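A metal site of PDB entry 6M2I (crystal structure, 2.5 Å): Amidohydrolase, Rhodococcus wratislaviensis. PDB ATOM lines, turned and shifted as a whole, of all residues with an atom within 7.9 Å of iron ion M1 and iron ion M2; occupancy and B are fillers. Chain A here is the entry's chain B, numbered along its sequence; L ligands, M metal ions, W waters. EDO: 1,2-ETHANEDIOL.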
ATOM      1  N   ALA A  24      16.217 -22.567  19.018  1.00  0.00           N
ATOM      2  CA  ALA A  24      16.443 -21.297  19.668  1.00  0.00           C
ATOM      3  C   ALA A  24      17.151 -20.285  18.780  1.00  0.00           C
ATOM      4  O   ALA A  24      17.036 -19.080  19.054  1.00  0.00           O
ATOM      5  CB  ALA A  24      17.243 -21.513  20.966  1.00  0.00           C
ATOM      6  N   ASP A  25      17.843 -20.699  17.724  1.00  0.00           N
ATOM      7  CA  ASP A  25      18.722 -19.775  16.993  1.00  0.00           C
ATOM      8  C   ASP A  25      18.562 -20.006  15.489  1.00  0.00           C
ATOM      9  O   ASP A  25      19.057 -21.009  14.956  1.00  0.00           O
ATOM     10  CB  ASP A  25      20.177 -19.932  17.434  1.00  0.00           C
ATOM     11  CG  ASP A  25      21.119 -18.931  16.780  1.00  0.00           C
ATOM     12  OD1 ASP A  25      20.693 -17.826  16.386  1.00  0.00           O
ATOM     13  OD2 ASP A  25      22.333 -19.221  16.656  1.00  0.00           O
ATOM     14  N   ILE A  26      17.844 -19.113  14.828  1.00  0.00           N
ATOM     15  CA  ILE A  26      17.654 -19.147  13.380  1.00  0.00           C
ATOM     16  C   ILE A  26      17.922 -17.754  12.855  1.00  0.00           C
ATOM     17  O   ILE A  26      17.389 -16.770  13.390  1.00  0.00           O
ATOM     18  CB  ILE A  26      16.239 -19.582  12.978  1.00  0.00           C
ATOM     19  CG1 ILE A  26      15.915 -20.976  13.506  1.00  0.00           C
ATOM     20  CG2 ILE A  26      16.065 -19.497  11.471  1.00  0.00           C
ATOM     21  CD1 ILE A  26      14.449 -21.277  13.436  1.00  0.00           C
ATOM     22  N   HIS A  27      18.740 -17.666  11.806  1.00  0.00           N
ATOM     23  CA  HIS A  27      19.147 -16.362  11.281  1.00  0.00           C
ATOM     24  C   HIS A  27      18.465 -16.099   9.961  1.00  0.00           C
ATOM     25  O   HIS A  27      18.926 -16.588   8.912  1.00  0.00           O
ATOM     26  CB  HIS A  27      20.661 -16.300  11.133  1.00  0.00           C
ATOM     27  CG  HIS A  27      21.372 -16.431  12.451  1.00  0.00           C
ATOM     28  ND1 HIS A  27      21.184 -15.537  13.480  1.00  0.00           N
ATOM     29  CD2 HIS A  27      22.193 -17.396  12.931  1.00  0.00           C
ATOM     30  CE1 HIS A  27      21.894 -15.926  14.520  1.00  0.00           C
ATOM     31  NE2 HIS A  27      22.511 -17.050  14.219  1.00  0.00           N
ATOM     32  N   GLN A 106      16.816 -14.522  15.052  1.00  0.00           N
ATOM     33  CA  GLN A 106      17.847 -13.691  15.677  1.00  0.00           C
ATOM     34  C   GLN A 106      18.584 -12.965  14.561  1.00  0.00           C
ATOM     35  O   GLN A 106      19.574 -13.479  14.028  1.00  0.00           O
ATOM     36  CB  GLN A 106      18.770 -14.541  16.534  1.00  0.00           C
ATOM     37  CG  GLN A 106      17.999 -15.180  17.668  1.00  0.00           C
ATOM     38  CD  GLN A 106      18.883 -15.815  18.697  1.00  0.00           C
ATOM     39  OE1 GLN A 106      20.090 -15.549  18.751  1.00  0.00           O
ATOM     40  NE2 GLN A 106      18.292 -16.652  19.543  1.00  0.00           N
ATOM     41  N   LEU A 108      20.855 -10.233  13.551  1.00  0.00           N
ATOM     42  CA  LEU A 108      21.864  -9.298  14.023  1.00  0.00           C
ATOM     43  C   LEU A 108      22.418  -8.390  12.918  1.00  0.00           C
ATOM     44  O   LEU A 108      22.927  -7.311  13.224  1.00  0.00           O
ATOM     45  CB  LEU A 108      23.024 -10.048  14.684  1.00  0.00           C
ATOM     46  CG  LEU A 108      22.791 -10.570  16.111  1.00  0.00           C
ATOM     47  CD1 LEU A 108      22.057  -9.563  16.997  1.00  0.00           C
ATOM     48  CD2 LEU A 108      22.063 -11.892  16.053  1.00  0.00           C
ATOM     49  N   HIS A 211      23.403 -13.423  22.076  1.00  0.00           N
ATOM     50  CA  HIS A 211      24.062 -14.142  21.006  1.00  0.00           C
ATOM     51  C   HIS A 211      25.539 -13.782  20.963  1.00  0.00           C
ATOM     52  O   HIS A 211      25.912 -12.631  21.165  1.00  0.00           O
ATOM     53  CB  HIS A 211      23.408 -13.808  19.672  1.00  0.00           C
ATOM     54  CG  HIS A 211      23.739 -14.777  18.581  1.00  0.00           C
ATOM     55  ND1 HIS A 211      24.906 -14.700  17.847  1.00  0.00           N
ATOM     56  CD2 HIS A 211      23.048 -15.818  18.070  1.00  0.00           C
ATOM     57  CE1 HIS A 211      24.921 -15.658  16.945  1.00  0.00           C
ATOM     58  NE2 HIS A 211      23.803 -16.356  17.053  1.00  0.00           N
ATOM     59  N   LEU A 212      26.370 -14.799  20.736  1.00  0.00           N
ATOM     60  CA  LEU A 212      27.750 -14.628  20.333  1.00  0.00           C
ATOM     61  C   LEU A 212      27.869 -13.453  19.385  1.00  0.00           C
ATOM     62  O   LEU A 212      27.123 -13.352  18.403  1.00  0.00           O
ATOM     63  CB  LEU A 212      28.248 -15.901  19.637  1.00  0.00           C
ATOM     64  CG  LEU A 212      29.620 -15.979  18.929  1.00  0.00           C
ATOM     65  CD1 LEU A 212      29.970 -17.441  18.637  1.00  0.00           C
ATOM     66  CD2 LEU A 212      29.689 -15.206  17.599  1.00  0.00           C
ATOM     67  N   HIS A 233      37.460 -18.080  16.848  1.00  0.00           N
ATOM     68  CA  HIS A 233      36.187 -18.760  17.000  1.00  0.00           C
ATOM     69  C   HIS A 233      36.111 -19.557  18.301  1.00  0.00           C
ATOM     70  O   HIS A 233      35.048 -19.622  18.916  1.00  0.00           O
ATOM     71  CB  HIS A 233      35.907 -19.642  15.793  1.00  0.00           C
ATOM     72  CG  HIS A 233      34.488 -20.090  15.704  1.00  0.00           C
ATOM     73  ND1 HIS A 233      34.065 -21.053  14.819  1.00  0.00           N
ATOM     74  CD2 HIS A 233      33.392 -19.721  16.406  1.00  0.00           C
ATOM     75  CE1 HIS A 233      32.775 -21.264  14.979  1.00  0.00           C
ATOM     76  NE2 HIS A 233      32.331 -20.470  15.937  1.00  0.00           N
ATOM     77  N   VAL A 264      23.709 -17.927  23.866  1.00  0.00           N
ATOM     78  CA  VAL A 264      23.377 -18.535  22.585  1.00  0.00           C
ATOM     79  C   VAL A 264      24.657 -18.603  21.761  1.00  0.00           C
ATOM     80  O   VAL A 264      25.295 -17.573  21.507  1.00  0.00           O
ATOM     81  CB  VAL A 264      22.296 -17.731  21.849  1.00  0.00           C
ATOM     82  CG1 VAL A 264      22.210 -18.187  20.410  1.00  0.00           C
ATOM     83  CG2 VAL A 264      20.967 -17.885  22.572  1.00  0.00           C
ATOM     84  N   GLU A 265      25.004 -19.819  21.340  1.00  0.00           N
ATOM     85  CA  GLU A 265      26.147 -20.064  20.475  1.00  0.00           C
ATOM     86  C   GLU A 265      27.449 -19.727  21.174  1.00  0.00           C
ATOM     87  O   GLU A 265      28.400 -19.258  20.545  1.00  0.00           O
ATOM     88  CB  GLU A 265      26.009 -19.300  19.159  1.00  0.00           C
ATOM     89  CG  GLU A 265      26.662 -19.987  17.981  1.00  0.00           C
ATOM     90  CD  GLU A 265      26.235 -19.357  16.687  1.00  0.00           C
ATOM     91  OE1 GLU A 265      25.070 -18.904  16.619  1.00  0.00           O
ATOM     92  OE2 GLU A 265      27.048 -19.293  15.740  1.00  0.00           O
ATOM     93  N   SER A 307      21.934 -22.488  24.787  1.00  0.00           N
ATOM     94  CA  SER A 307      21.618 -23.274  23.613  1.00  0.00           C
ATOM     95  C   SER A 307      22.799 -24.187  23.251  1.00  0.00           C
ATOM     96  O   SER A 307      23.932 -23.964  23.667  1.00  0.00           O
ATOM     97  CB  SER A 307      21.256 -22.357  22.438  1.00  0.00           C
ATOM     98  OG  SER A 307      22.391 -21.664  21.943  1.00  0.00           O
ATOM     99  N   GLN A 309      24.009 -25.345  19.996  1.00  0.00           N
ATOM    100  CA  GLN A 309      24.895 -25.183  18.859  1.00  0.00           C
ATOM    101  C   GLN A 309      26.035 -24.224  19.210  1.00  0.00           C
ATOM    102  O   GLN A 309      25.820 -23.224  19.914  1.00  0.00           O
ATOM    103  CB  GLN A 309      24.112 -24.665  17.654  1.00  0.00           C
ATOM    104  CG  GLN A 309      24.835 -24.822  16.334  1.00  0.00           C
ATOM    105  CD  GLN A 309      25.688 -23.611  16.027  1.00  0.00           C
ATOM    106  OE1 GLN A 309      25.485 -22.552  16.619  1.00  0.00           O
ATOM    107  NE2 GLN A 309      26.646 -23.762  15.088  1.00  0.00           N
ATOM    108  N   PRO A 310      27.276 -24.513  18.784  1.00  0.00           N
ATOM    109  CA  PRO A 310      27.721 -25.777  18.181  1.00  0.00           C
ATOM    110  C   PRO A 310      27.970 -26.801  19.258  1.00  0.00           C
ATOM    111  O   PRO A 310      28.650 -26.495  20.227  1.00  0.00           O
ATOM    112  CB  PRO A 310      29.030 -25.406  17.464  1.00  0.00           C
ATOM    113  CG  PRO A 310      29.566 -24.250  18.281  1.00  0.00           C
ATOM    114  CD  PRO A 310      28.357 -23.509  18.838  1.00  0.00           C
ATOM    115  N   ALA A 335      19.284 -25.713  19.296  1.00  0.00           N
ATOM    116  CA  ALA A 335      19.293 -24.699  18.241  1.00  0.00           C
ATOM    117  C   ALA A 335      20.032 -25.245  17.028  1.00  0.00           C
ATOM    118  O   ALA A 335      20.995 -26.019  17.150  1.00  0.00           O
ATOM    119  CB  ALA A 335      19.931 -23.394  18.717  1.00  0.00           C
ATOM    120  N   THR A 336      19.588 -24.823  15.838  1.00  0.00           N
ATOM    121  CA  THR A 336      20.270 -25.223  14.615  1.00  0.00           C
ATOM    122  C   THR A 336      21.354 -24.240  14.192  1.00  0.00           C
ATOM    123  O   THR A 336      22.379 -24.666  13.651  1.00  0.00           O
ATOM    124  CB  THR A 336      19.279 -25.339  13.441  1.00  0.00           C
ATOM    125  OG1 THR A 336      18.676 -24.059  13.205  1.00  0.00           O
ATOM    126  CG2 THR A 336      18.206 -26.400  13.680  1.00  0.00           C
ATOM    127  N   ASP A 337      21.117 -22.937  14.411  1.00  0.00           N
ATOM    128  CA  ASP A 337      21.953 -21.871  13.838  1.00  0.00           C
ATOM    129  C   ASP A 337      21.858 -21.869  12.315  1.00  0.00           C
ATOM    130  O   ASP A 337      22.795 -21.443  11.620  1.00  0.00           O
ATOM    131  CB  ASP A 337      23.405 -21.986  14.296  1.00  0.00           C
ATOM    132  CG  ASP A 337      24.159 -20.679  14.157  1.00  0.00           C
ATOM    133  OD1 ASP A 337      23.499 -19.639  14.035  1.00  0.00           O
ATOM    134  OD2 ASP A 337      25.405 -20.695  14.165  1.00  0.00           O
ATOM    135  N   TYR A 338      20.737 -22.324  11.792  1.00  0.00           N
ATOM    136  CA  TYR A 338      20.505 -22.302  10.364  1.00  0.00           C
ATOM    137  C   TYR A 338      20.494 -20.863   9.879  1.00  0.00           C
ATOM    138  O   TYR A 338      19.848 -20.009  10.493  1.00  0.00           O
ATOM    139  CB  TYR A 338      19.177 -23.001  10.032  1.00  0.00           C
ATOM    140  CG  TYR A 338      18.812 -23.004   8.561  1.00  0.00           C
ATOM    141  CD1 TYR A 338      18.184 -21.912   7.982  1.00  0.00           C
ATOM    142  CD2 TYR A 338      19.117 -24.090   7.750  1.00  0.00           C
ATOM    143  CE1 TYR A 338      17.865 -21.897   6.626  1.00  0.00           C
ATOM    144  CE2 TYR A 338      18.806 -24.090   6.399  1.00  0.00           C
ATOM    145  CZ  TYR A 338      18.179 -22.997   5.852  1.00  0.00           C
ATOM    146  OH  TYR A 338      17.856 -22.985   4.518  1.00  0.00           O
ATOM    147  N   PRO A 339      21.152 -20.556   8.751  1.00  0.00           N
ATOM    148  CA  PRO A 339      21.822 -21.484   7.833  1.00  0.00           C
ATOM    149  C   PRO A 339      23.356 -21.488   7.863  1.00  0.00           C
ATOM    150  O   PRO A 339      23.963 -21.647   6.810  1.00  0.00           O
ATOM    151  CB  PRO A 339      21.327 -20.997   6.471  1.00  0.00           C
ATOM    152  CG  PRO A 339      21.250 -19.496   6.656  1.00  0.00           C
ATOM    153  CD  PRO A 339      21.003 -19.226   8.130  1.00  0.00           C
ATOM    154  N   HIS A 340      23.969 -21.341   9.031  1.00  0.00           N
ATOM    155  CA  HIS A 340      25.426 -21.247   9.104  1.00  0.00           C
ATOM    156  C   HIS A 340      26.101 -22.584   8.811  1.00  0.00           C
ATOM    157  O   HIS A 340      25.502 -23.658   8.964  1.00  0.00           O
ATOM    158  CB  HIS A 340      25.857 -20.762  10.492  1.00  0.00           C
ATOM    159  CG  HIS A 340      25.506 -19.335  10.750  1.00  0.00           C
ATOM    160  ND1 HIS A 340      25.963 -18.653  11.853  1.00  0.00           N
ATOM    161  CD2 HIS A 340      24.752 -18.471  10.043  1.00  0.00           C
ATOM    162  CE1 HIS A 340      25.496 -17.414  11.820  1.00  0.00           C
ATOM    163  NE2 HIS A 340      24.757 -17.277  10.731  1.00  0.00           N
ATOM    164  N   PHE A 341      27.390 -22.509   8.451  1.00  0.00           N
ATOM    165  CA  PHE A 341      28.131 -23.694   8.022  1.00  0.00           C
ATOM    166  C   PHE A 341      28.210 -24.736   9.133  1.00  0.00           C
ATOM    167  O   PHE A 341      28.097 -25.942   8.871  1.00  0.00           O
ATOM    168  CB  PHE A 341      29.540 -23.302   7.538  1.00  0.00           C
ATOM    169  CG  PHE A 341      30.593 -23.276   8.622  1.00  0.00           C
ATOM    170  CD1 PHE A 341      30.832 -22.103   9.365  1.00  0.00           C
ATOM    171  CD2 PHE A 341      31.376 -24.404   8.889  1.00  0.00           C
ATOM    172  CE1 PHE A 341      31.815 -22.072  10.369  1.00  0.00           C
ATOM    173  CE2 PHE A 341      32.355 -24.382   9.891  1.00  0.00           C
ATOM    174  CZ  PHE A 341      32.579 -23.212  10.626  1.00  0.00           C
ATOM    175  N   ASP A 342      28.387 -24.300  10.379  1.00  0.00           N
ATOM    176  CA  ASP A 342      28.455 -25.219  11.504  1.00  0.00           C
ATOM    177  C   ASP A 342      27.089 -25.523  12.096  1.00  0.00           C
ATOM    178  O   ASP A 342      26.989 -25.849  13.289  1.00  0.00           O
ATOM    179  CB  ASP A 342      29.388 -24.658  12.591  1.00  0.00           C
ATOM    180  CG  ASP A 342      29.004 -23.242  12.983  1.00  0.00           C
ATOM    181  OD1 ASP A 342      28.013 -22.711  12.432  1.00  0.00           O
ATOM    182  OD2 ASP A 342      29.718 -22.667  13.844  1.00  0.00           O
ATOM    183  N   PHE A 343      26.030 -25.419  11.289  1.00  0.00           N
ATOM    184  CA  PHE A 343      24.689 -25.656  11.801  1.00  0.00           C
ATOM    185  C   PHE A 343      24.529 -27.100  12.271  1.00  0.00           C
ATOM    186  O   PHE A 343      25.189 -28.015  11.784  1.00  0.00           O
ATOM    187  CB  PHE A 343      23.648 -25.303  10.730  1.00  0.00           C
ATOM    188  CG  PHE A 343      23.117 -26.492   9.987  1.00  0.00           C
ATOM    189  CD1 PHE A 343      23.745 -26.933   8.838  1.00  0.00           C
ATOM    190  CD2 PHE A 343      21.974 -27.144  10.422  1.00  0.00           C
ATOM    191  CE1 PHE A 343      23.268 -28.015   8.153  1.00  0.00           C
ATOM    192  CE2 PHE A 343      21.483 -28.232   9.737  1.00  0.00           C
ATOM    193  CZ  PHE A 343      22.129 -28.674   8.606  1.00  0.00           C
HETATM  194  C1  EDO L   1      29.689 -18.324  13.607  1.00  0.00           C
HETATM  195  O1  EDO L   1      28.670 -17.330  13.665  1.00  0.00           O
HETATM  196  C2  EDO L   1      29.250 -19.427  12.644  1.00  0.00           C
HETATM  197  O2  EDO L   1      28.230 -20.263  13.212  1.00  0.00           O
HETATM  198 FE    FE M   1      26.443 -18.966  13.803  1.00  0.00          FE
HETATM  199 FE    FE M   2      23.742 -18.054  15.491  1.00  0.00          FE
HETATM  200  O   HOH W   1      25.778 -17.144  14.605  1.00  0.00           O
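N of His 27 lies within hydrogen-bond range of O of Tyr 338 (2.9 Å).
The side-chain amide oxygen of Gln 309 sits close to the side-chain carboxylate of Asp 337, at 3.1 Å.
The side-chain carboxylate of Asp 25 sits close to the side-chain amide oxygen of Gln 106 (3.3 Å).
A ring nitrogen (ND1) of His 27 is in hydrogen-bond range of the backbone carbonyl oxygen (O) of Gln 106 (2.7 Å).
OG of Ser 307 is in hydrogen-bond range of N of Glu 265.
Three residues have an atom within 4 Å of iron ion M1: Glu 265, Asp 337 and His 340.
The nearest printed residue that does not touch iron ion M2 is His 340 (4.1 Å).
Iron ion M1 is bound by a ring nitrogen (ND1) of His 340 (2.0 Å), the side-chain carboxylate (OD2) of Asp 337 (2.0 Å), the side-chain carboxylate (OE2) of Glu 265 (2.1 Å), water W1 (2.1 Å) and an oxygen (O2) of the ligand (2.3 Å).
Iron ion M1 has five donor atoms within binding distance.
Slightly farther from iron ion M1 lies an oxygen (O1) of the ligand (2.8 Å).
Iron ion M2 is bound by OE1 of Glu 265, NE2 of His 27, OD1 of Asp 337, OD2 of Asp 25, NE2 of His 211 and water W1.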
